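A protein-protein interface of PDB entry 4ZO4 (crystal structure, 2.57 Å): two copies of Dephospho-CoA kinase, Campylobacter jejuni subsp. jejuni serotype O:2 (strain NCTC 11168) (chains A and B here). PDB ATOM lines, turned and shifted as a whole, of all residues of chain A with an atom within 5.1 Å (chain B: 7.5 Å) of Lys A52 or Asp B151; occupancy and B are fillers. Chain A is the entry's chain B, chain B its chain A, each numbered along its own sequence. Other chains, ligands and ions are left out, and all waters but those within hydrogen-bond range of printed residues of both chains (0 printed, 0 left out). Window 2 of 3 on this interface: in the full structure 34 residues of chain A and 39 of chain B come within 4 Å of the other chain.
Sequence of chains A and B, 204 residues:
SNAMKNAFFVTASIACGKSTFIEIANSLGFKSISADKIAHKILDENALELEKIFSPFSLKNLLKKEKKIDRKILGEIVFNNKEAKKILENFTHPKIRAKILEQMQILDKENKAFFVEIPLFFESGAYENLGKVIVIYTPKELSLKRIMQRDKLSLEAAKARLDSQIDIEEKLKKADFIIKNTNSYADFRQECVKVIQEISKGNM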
ATOM      1  N   LEU A  48      17.141 -33.706  16.656  1.00  0.00           N
ATOM      2  CA  LEU A  48      16.699 -32.380  16.217  1.00  0.00           C
ATOM      3  C   LEU A  48      16.849 -32.188  14.731  1.00  0.00           C
ATOM      4  O   LEU A  48      15.934 -31.715  14.063  1.00  0.00           O
ATOM      5  CB  LEU A  48      17.458 -31.245  16.910  1.00  0.00           C
ATOM      6  CG  LEU A  48      17.357 -31.081  18.432  1.00  0.00           C
ATOM      7  CD1 LEU A  48      17.995 -29.760  18.859  1.00  0.00           C
ATOM      8  CD2 LEU A  48      15.921 -31.165  18.925  1.00  0.00           C
ATOM      9  N   GLU A  49      18.012 -32.532  14.204  1.00  0.00           N
ATOM     10  CA  GLU A  49      18.247 -32.369  12.773  1.00  0.00           C
ATOM     11  C   GLU A  49      17.333 -33.300  11.973  1.00  0.00           C
ATOM     12  O   GLU A  49      16.856 -32.959  10.889  1.00  0.00           O
ATOM     13  CB  GLU A  49      19.728 -32.562  12.451  1.00  0.00           C
ATOM     14  CG  GLU A  49      20.630 -31.787  13.420  1.00  0.00           C
ATOM     15  CD  GLU A  49      21.809 -31.085  12.774  1.00  0.00           C
ATOM     16  OE1 GLU A  49      22.705 -31.766  12.255  1.00  0.00           O
ATOM     17  OE2 GLU A  49      21.855 -29.835  12.820  1.00  0.00           O
ATOM     18  N   LEU A  50      17.034 -34.459  12.529  1.00  0.00           N
ATOM     19  CA  LEU A  50      16.218 -35.401  11.807  1.00  0.00           C
ATOM     20  C   LEU A  50      14.825 -34.903  11.618  1.00  0.00           C
ATOM     21  O   LEU A  50      14.240 -35.214  10.608  1.00  0.00           O
ATOM     22  CB  LEU A  50      16.141 -36.743  12.513  1.00  0.00           C
ATOM     23  CG  LEU A  50      17.372 -37.597  12.381  1.00  0.00           C
ATOM     24  CD1 LEU A  50      17.085 -38.876  13.125  1.00  0.00           C
ATOM     25  CD2 LEU A  50      17.685 -37.851  10.933  1.00  0.00           C
ATOM     26  N   GLU A  51      14.279 -34.176  12.603  1.00  0.00           N
ATOM     27  CA  GLU A  51      12.922 -33.685  12.490  1.00  0.00           C
ATOM     28  C   GLU A  51      12.908 -32.600  11.448  1.00  0.00           C
ATOM     29  O   GLU A  51      11.972 -32.521  10.662  1.00  0.00           O
ATOM     30  CB  GLU A  51      12.267 -33.301  13.838  1.00  0.00           C
ATOM     31  CG  GLU A  51      12.562 -31.925  14.441  1.00  0.00           C
ATOM     32  CD  GLU A  51      11.710 -30.780  13.915  1.00  0.00           C
ATOM     33  OE1 GLU A  51      12.147 -29.616  14.067  1.00  0.00           O
ATOM     34  OE2 GLU A  51      10.614 -31.014  13.358  1.00  0.00           O
ATOM     35  N   LYS A  52      13.966 -31.817  11.370  1.00  0.00           N
ATOM     36  CA  LYS A  52      14.023 -30.759  10.362  1.00  0.00           C
ATOM     37  C   LYS A  52      14.192 -31.306   8.957  1.00  0.00           C
ATOM     38  O   LYS A  52      13.676 -30.726   8.002  1.00  0.00           O
ATOM     39  CB  LYS A  52      15.135 -29.748  10.677  1.00  0.00           C
ATOM     40  CG  LYS A  52      14.673 -28.645  11.628  1.00  0.00           C
ATOM     41  CD  LYS A  52      15.829 -27.963  12.352  1.00  0.00           C
ATOM     42  CE  LYS A  52      15.363 -27.308  13.645  1.00  0.00           C
ATOM     43  NZ  LYS A  52      16.525 -26.815  14.436  1.00  0.00           N
ATOM     44  N   ILE A  53      14.941 -32.404   8.808  1.00  0.00           N
ATOM     45  CA  ILE A  53      15.040 -33.048   7.488  1.00  0.00           C
ATOM     46  C   ILE A  53      13.705 -33.687   7.140  1.00  0.00           C
ATOM     47  O   ILE A  53      13.243 -33.544   6.025  1.00  0.00           O
ATOM     48  CB  ILE A  53      16.133 -34.109   7.414  1.00  0.00           C
ATOM     49  CG1 ILE A  53      17.519 -33.491   7.695  1.00  0.00           C
ATOM     50  CG2 ILE A  53      16.156 -34.738   6.038  1.00  0.00           C
ATOM     51  CD1 ILE A  53      18.441 -34.381   8.502  1.00  0.00           C
ATOM     52  N   PHE A  54      13.090 -34.373   8.097  1.00  0.00           N
ATOM     53  CA  PHE A  54      11.962 -35.211   7.789  1.00  0.00           C
ATOM     54  C   PHE A  54      10.573 -34.612   8.044  1.00  0.00           C
ATOM     55  O   PHE A  54       9.588 -35.216   7.638  1.00  0.00           O
ATOM     56  CB  PHE A  54      12.135 -36.616   8.408  1.00  0.00           C
ATOM     57  CG  PHE A  54      13.182 -37.469   7.682  1.00  0.00           C
ATOM     58  CD1 PHE A  54      12.864 -38.140   6.486  1.00  0.00           C
ATOM     59  CD2 PHE A  54      14.476 -37.563   8.157  1.00  0.00           C
ATOM     60  CE1 PHE A  54      13.802 -38.906   5.795  1.00  0.00           C
ATOM     61  CE2 PHE A  54      15.427 -38.325   7.478  1.00  0.00           C
ATOM     62  CZ  PHE A  54      15.092 -38.991   6.288  1.00  0.00           C
ATOM     63  N   SER A  55      10.455 -33.417   8.620  1.00  0.00           N
ATOM     64  CA  SER A  55       9.114 -32.882   8.851  1.00  0.00           C
ATOM     65  C   SER A  55       8.318 -32.670   7.538  1.00  0.00           C
ATOM     66  O   SER A  55       7.112 -32.938   7.516  1.00  0.00           O
ATOM     67  CB  SER A  55       9.117 -31.614   9.708  1.00  0.00           C
ATOM     68  OG  SER A  55       9.754 -30.543   9.047  1.00  0.00           O
ATOM     69  N   PRO A  56       8.977 -32.257   6.430  1.00  0.00           N
ATOM     70  CA  PRO A  56       8.174 -32.200   5.190  1.00  0.00           C
ATOM     71  C   PRO A  56       7.685 -33.543   4.601  1.00  0.00           C
ATOM     72  O   PRO A  56       6.927 -33.526   3.633  1.00  0.00           O
ATOM     73  CB  PRO A  56       9.107 -31.518   4.183  1.00  0.00           C
ATOM     74  CG  PRO A  56      10.478 -31.585   4.769  1.00  0.00           C
ATOM     75  CD  PRO A  56      10.312 -31.656   6.252  1.00  0.00           C
ATOM     76  N   LYS B 140      12.047 -24.036  -3.780  1.00  0.00           N
ATOM     77  CA  LYS B 140      13.029 -23.862  -2.693  1.00  0.00           C
ATOM     78  C   LYS B 140      14.351 -23.374  -3.238  1.00  0.00           C
ATOM     79  O   LYS B 140      14.699 -23.647  -4.384  1.00  0.00           O
ATOM     80  CB  LYS B 140      13.281 -25.178  -1.967  1.00  0.00           C
ATOM     81  CG  LYS B 140      12.099 -25.687  -1.166  1.00  0.00           C
ATOM     82  CD  LYS B 140      11.852 -24.854   0.071  1.00  0.00           C
ATOM     83  CE  LYS B 140      10.809 -25.532   0.930  1.00  0.00           C
ATOM     84  NZ  LYS B 140      10.592 -24.762   2.178  1.00  0.00           N
ATOM     85  N   GLU B 141      15.104 -22.642  -2.426  1.00  0.00           N
ATOM     86  CA  GLU B 141      16.432 -22.237  -2.874  1.00  0.00           C
ATOM     87  C   GLU B 141      17.349 -23.459  -2.743  1.00  0.00           C
ATOM     88  O   GLU B 141      17.491 -24.061  -1.658  1.00  0.00           O
ATOM     89  CB  GLU B 141      16.972 -21.022  -2.120  1.00  0.00           C
ATOM     90  CG  GLU B 141      17.655 -20.013  -3.057  1.00  0.00           C
ATOM     91  CD  GLU B 141      18.496 -18.977  -2.317  1.00  0.00           C
ATOM     92  OE1 GLU B 141      18.722 -17.880  -2.874  1.00  0.00           O
ATOM     93  OE2 GLU B 141      18.935 -19.257  -1.180  1.00  0.00           O
ATOM     94  N   LYS B 145      24.263 -23.005   1.481  1.00  0.00           N
ATOM     95  CA  LYS B 145      24.659 -22.080   2.553  1.00  0.00           C
ATOM     96  C   LYS B 145      23.436 -21.369   3.124  1.00  0.00           C
ATOM     97  O   LYS B 145      23.328 -21.147   4.334  1.00  0.00           O
ATOM     98  CB  LYS B 145      25.667 -21.016   2.064  1.00  0.00           C
ATOM     99  CG  LYS B 145      26.637 -21.409   0.940  1.00  0.00           C
ATOM    100  CD  LYS B 145      27.707 -22.396   1.392  1.00  0.00           C
ATOM    101  CE  LYS B 145      28.931 -22.333   0.492  1.00  0.00           C
ATOM    102  NZ  LYS B 145      30.184 -22.500   1.277  1.00  0.00           N
ATOM    103  N   ARG B 146      22.512 -21.021   2.240  1.00  0.00           N
ATOM    104  CA  ARG B 146      21.278 -20.411   2.659  1.00  0.00           C
ATOM    105  C   ARG B 146      20.388 -21.375   3.449  1.00  0.00           C
ATOM    106  O   ARG B 146      19.492 -20.939   4.148  1.00  0.00           O
ATOM    107  CB  ARG B 146      20.536 -19.824   1.449  1.00  0.00           C
ATOM    108  CG  ARG B 146      21.208 -18.598   0.798  1.00  0.00           C
ATOM    109  CD  ARG B 146      21.320 -17.394   1.736  1.00  0.00           C
ATOM    110  NE  ARG B 146      20.977 -16.119   1.095  1.00  0.00           N
ATOM    111  CZ  ARG B 146      19.737 -15.613   0.988  1.00  0.00           C
ATOM    112  NH1 ARG B 146      18.679 -16.273   1.456  1.00  0.00           N
ATOM    113  NH2 ARG B 146      19.547 -14.437   0.393  1.00  0.00           N
ATOM    114  N   ILE B 147      20.618 -22.677   3.341  1.00  0.00           N
ATOM    115  CA  ILE B 147      19.862 -23.645   4.139  1.00  0.00           C
ATOM    116  C   ILE B 147      20.424 -23.784   5.562  1.00  0.00           C
ATOM    117  O   ILE B 147      19.669 -23.994   6.518  1.00  0.00           O
ATOM    118  CB  ILE B 147      19.817 -25.028   3.455  1.00  0.00           C
ATOM    119  CG1 ILE B 147      19.024 -24.956   2.137  1.00  0.00           C
ATOM    120  CG2 ILE B 147      19.185 -26.062   4.382  1.00  0.00           C
ATOM    121  CD1 ILE B 147      19.125 -26.204   1.275  1.00  0.00           C
ATOM    122  N   MET B 148      21.739 -23.689   5.704  1.00  0.00           N
ATOM    123  CA  MET B 148      22.395 -23.770   7.026  1.00  0.00           C
ATOM    124  C   MET B 148      22.026 -22.568   7.859  1.00  0.00           C
ATOM    125  O   MET B 148      21.663 -22.732   9.006  1.00  0.00           O
ATOM    126  CB  MET B 148      23.925 -23.904   6.928  1.00  0.00           C
ATOM    127  CG  MET B 148      24.314 -25.288   6.433  1.00  0.00           C
ATOM    128  SD  MET B 148      26.142 -25.300   5.707  1.00  0.00           S
ATOM    129  CE  MET B 148      27.106 -25.266   7.418  1.00  0.00           C
ATOM    130  N   GLN B 149      22.114 -21.366   7.281  1.00  0.00           N
ATOM    131  CA  GLN B 149      21.647 -20.121   7.939  1.00  0.00           C
ATOM    132  C   GLN B 149      20.186 -20.204   8.385  1.00  0.00           C
ATOM    133  O   GLN B 149      19.899 -20.316   9.568  1.00  0.00           O
ATOM    134  CB  GLN B 149      21.752 -18.906   6.998  1.00  0.00           C
ATOM    135  CG  GLN B 149      23.151 -18.502   6.557  1.00  0.00           C
ATOM    136  CD  GLN B 149      23.144 -17.460   5.431  1.00  0.00           C
ATOM    137  OE1 GLN B 149      22.083 -17.027   4.952  1.00  0.00           O
ATOM    138  NE2 GLN B 149      24.337 -17.060   4.998  1.00  0.00           N
ATOM    139  N   ARG B 150      19.276 -20.153   7.413  1.00  0.00           N
ATOM    140  CA  ARG B 150      17.838 -20.090   7.654  1.00  0.00           C
ATOM    141  C   ARG B 150      17.362 -21.226   8.552  1.00  0.00           C
ATOM    142  O   ARG B 150      16.676 -20.992   9.543  1.00  0.00           O
ATOM    143  CB  ARG B 150      17.095 -20.133   6.306  1.00  0.00           C
ATOM    144  CG  ARG B 150      15.588 -20.345   6.387  1.00  0.00           C
ATOM    145  CD  ARG B 150      14.808 -19.049   6.420  1.00  0.00           C
ATOM    146  NE  ARG B 150      13.468 -19.259   6.975  1.00  0.00           N
ATOM    147  CZ  ARG B 150      12.441 -19.821   6.330  1.00  0.00           C
ATOM    148  NH1 ARG B 150      11.265 -19.946   6.946  1.00  0.00           N
ATOM    149  NH2 ARG B 150      12.570 -20.265   5.079  1.00  0.00           N
ATOM    150  N   ASP B 151      17.732 -22.456   8.203  1.00  0.00           N
ATOM    151  CA  ASP B 151      17.178 -23.628   8.868  1.00  0.00           C
ATOM    152  C   ASP B 151      18.040 -24.084  10.036  1.00  0.00           C
ATOM    153  O   ASP B 151      17.676 -25.033  10.727  1.00  0.00           O
ATOM    154  CB  ASP B 151      16.925 -24.754   7.850  1.00  0.00           C
ATOM    155  CG  ASP B 151      16.033 -24.300   6.658  1.00  0.00           C
ATOM    156  OD1 ASP B 151      15.353 -23.259   6.787  1.00  0.00           O
ATOM    157  OD2 ASP B 151      15.982 -24.993   5.603  1.00  0.00           O
ATOM    158  N   LYS B 152      19.167 -23.398  10.269  1.00  0.00           N
ATOM    159  CA  LYS B 152      20.064 -23.667  11.428  1.00  0.00           C
ATOM    160  C   LYS B 152      20.611 -25.108  11.497  1.00  0.00           C
ATOM    161  O   LYS B 152      20.490 -25.789  12.524  1.00  0.00           O
ATOM    162  CB  LYS B 152      19.378 -23.291  12.761  1.00  0.00           C
ATOM    163  CG  LYS B 152      19.924 -22.037  13.435  1.00  0.00           C
ATOM    164  CD  LYS B 152      19.254 -20.762  12.935  1.00  0.00           C
ATOM    165  CE  LYS B 152      19.996 -19.524  13.426  1.00  0.00           C
ATOM    166  NZ  LYS B 152      19.453 -18.275  12.827  1.00  0.00           N
ATOM    167  N   LEU B 153      21.227 -25.565  10.410  1.00  0.00           N
ATOM    168  CA  LEU B 153      21.692 -26.969  10.331  1.00  0.00           C
ATOM    169  C   LEU B 153      23.177 -27.098  10.049  1.00  0.00           C
ATOM    170  O   LEU B 153      23.830 -26.180   9.598  1.00  0.00           O
ATOM    171  CB  LEU B 153      20.935 -27.751   9.248  1.00  0.00           C
ATOM    172  CG  LEU B 153      19.407 -27.645   9.196  1.00  0.00           C
ATOM    173  CD1 LEU B 153      18.915 -27.728   7.758  1.00  0.00           C
ATOM    174  CD2 LEU B 153      18.758 -28.724  10.054  1.00  0.00           C
ATOM    175  N   SER B 154      23.694 -28.273  10.347  1.00  0.00           N
ATOM    176  CA  SER B 154      25.040 -28.655   9.961  1.00  0.00           C
ATOM    177  C   SER B 154      25.107 -28.966   8.463  1.00  0.00           C
ATOM    178  O   SER B 154      24.088 -29.177   7.789  1.00  0.00           O
ATOM    179  CB  SER B 154      25.444 -29.892  10.740  1.00  0.00           C
ATOM    180  OG  SER B 154      24.450 -30.889  10.592  1.00  0.00           O
ATOM    181  N   ALA B 157      23.172 -32.324   7.565  1.00  0.00           N
ATOM    182  CA  ALA B 157      21.724 -32.249   7.475  1.00  0.00           C
ATOM    183  C   ALA B 157      21.272 -31.331   6.298  1.00  0.00           C
ATOM    184  O   ALA B 157      20.258 -31.584   5.625  1.00  0.00           O
ATOM    185  CB  ALA B 157      21.158 -31.761   8.790  1.00  0.00           C
ATOM    186  N   ALA B 158      22.038 -30.285   6.037  1.00  0.00           N
ATOM    187  CA  ALA B 158      21.741 -29.426   4.916  1.00  0.00           C
ATOM    188  C   ALA B 158      21.836 -30.212   3.619  1.00  0.00           C
ATOM    189  O   ALA B 158      21.015 -30.050   2.705  1.00  0.00           O
ATOM    190  CB  ALA B 158      22.688 -28.249   4.905  1.00  0.00           C
ATOM    191  N   ARG B 161      18.708 -32.271   3.154  1.00  0.00           N
ATOM    192  CA  ARG B 161      17.603 -31.486   2.820  1.00  0.00           C
ATOM    193  C   ARG B 161      17.697 -31.053   1.371  1.00  0.00           C
ATOM    194  O   ARG B 161      16.723 -31.133   0.622  1.00  0.00           O
ATOM    195  CB  ARG B 161      17.542 -30.272   3.749  1.00  0.00           C
ATOM    196  CG  ARG B 161      16.142 -29.702   3.779  1.00  0.00           C
ATOM    197  CD  ARG B 161      15.933 -28.777   4.931  1.00  0.00           C
ATOM    198  NE  ARG B 161      14.595 -28.934   5.491  1.00  0.00           N
ATOM    199  CZ  ARG B 161      14.022 -28.032   6.280  1.00  0.00           C
ATOM    200  NH1 ARG B 161      14.659 -26.903   6.585  1.00  0.00           N
ATOM    201  NH2 ARG B 161      12.800 -28.248   6.755  1.00  0.00           N
ATOM    202  N   GLN B 165      15.181 -31.933  -1.934  1.00  0.00           N
ATOM    203  CA  GLN B 165      14.627 -30.866  -2.773  1.00  0.00           C
ATOM    204  C   GLN B 165      15.022 -31.044  -4.217  1.00  0.00           C
ATOM    205  O   GLN B 165      14.183 -30.950  -5.095  1.00  0.00           O
ATOM    206  CB  GLN B 165      15.041 -29.498  -2.273  1.00  0.00           C
ATOM    207  CG  GLN B 165      14.457 -29.166  -0.899  1.00  0.00           C
ATOM    208  CD  GLN B 165      15.083 -27.918  -0.276  1.00  0.00           C
ATOM    209  OE1 GLN B 165      15.684 -27.092  -0.968  1.00  0.00           O
ATOM    210  NE2 GLN B 165      14.942 -27.777   1.040  1.00  0.00           N
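The side-chain carboxylate (OE1) of Glu A49 is in hydrogen-bond range of the side-chain hydroxyl (OG) of Ser B154.
O of Lys A52 lies within hydrogen-bond range of NH2 of Arg B161, at 2.9 Å.
The side-chain carboxylate (OD2) of Asp B151 lies within salt-bridge range of the guanidinium group (NH1) of Arg B161, 2.5 Å away.
The backbone carbonyl oxygen (O) of Met B148 sits at hydrogen-bond distance from the backbone NH (N) of Leu B153.
Among the printed residues, pairs that only touch across the chains: Glu A49 with Leu B153, Glu A49 with Ala B157, Lys A52 with Asp B151, Lys A52 with Leu B153 and Ile A53 with Ala B157.
Lys A52 touches just these residues of chain B: Asp B151 (3.8 Å), Leu B153 (3.8 Å) and Arg B161 (2.9 Å).
Asp B151 touches just one residue of chain A: Lys A52 (3.8 Å).
Of the printed residues of chain B, Glu A49 touches Leu B153, Ser B154 and Ala B157.
Of the printed residues of chain B, Ile A53 touches Ala B157.
Hydrophobic or aromatic side chains of chain A within 4 Å of the printed part of chain B: Ile A53.
Of the 16 printed residues of chain B, 5 touch a printed residue of chain A.
Hydrophobic or aromatic side chains of chain B that line the printed part of chain A: Leu B153 and Ala B157.
Among the printed residues, no Asp or Glu carboxylate lies within 4 Å of a Lys or Arg side-chain nitrogen of the other chain.
No position is printed for both chains.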
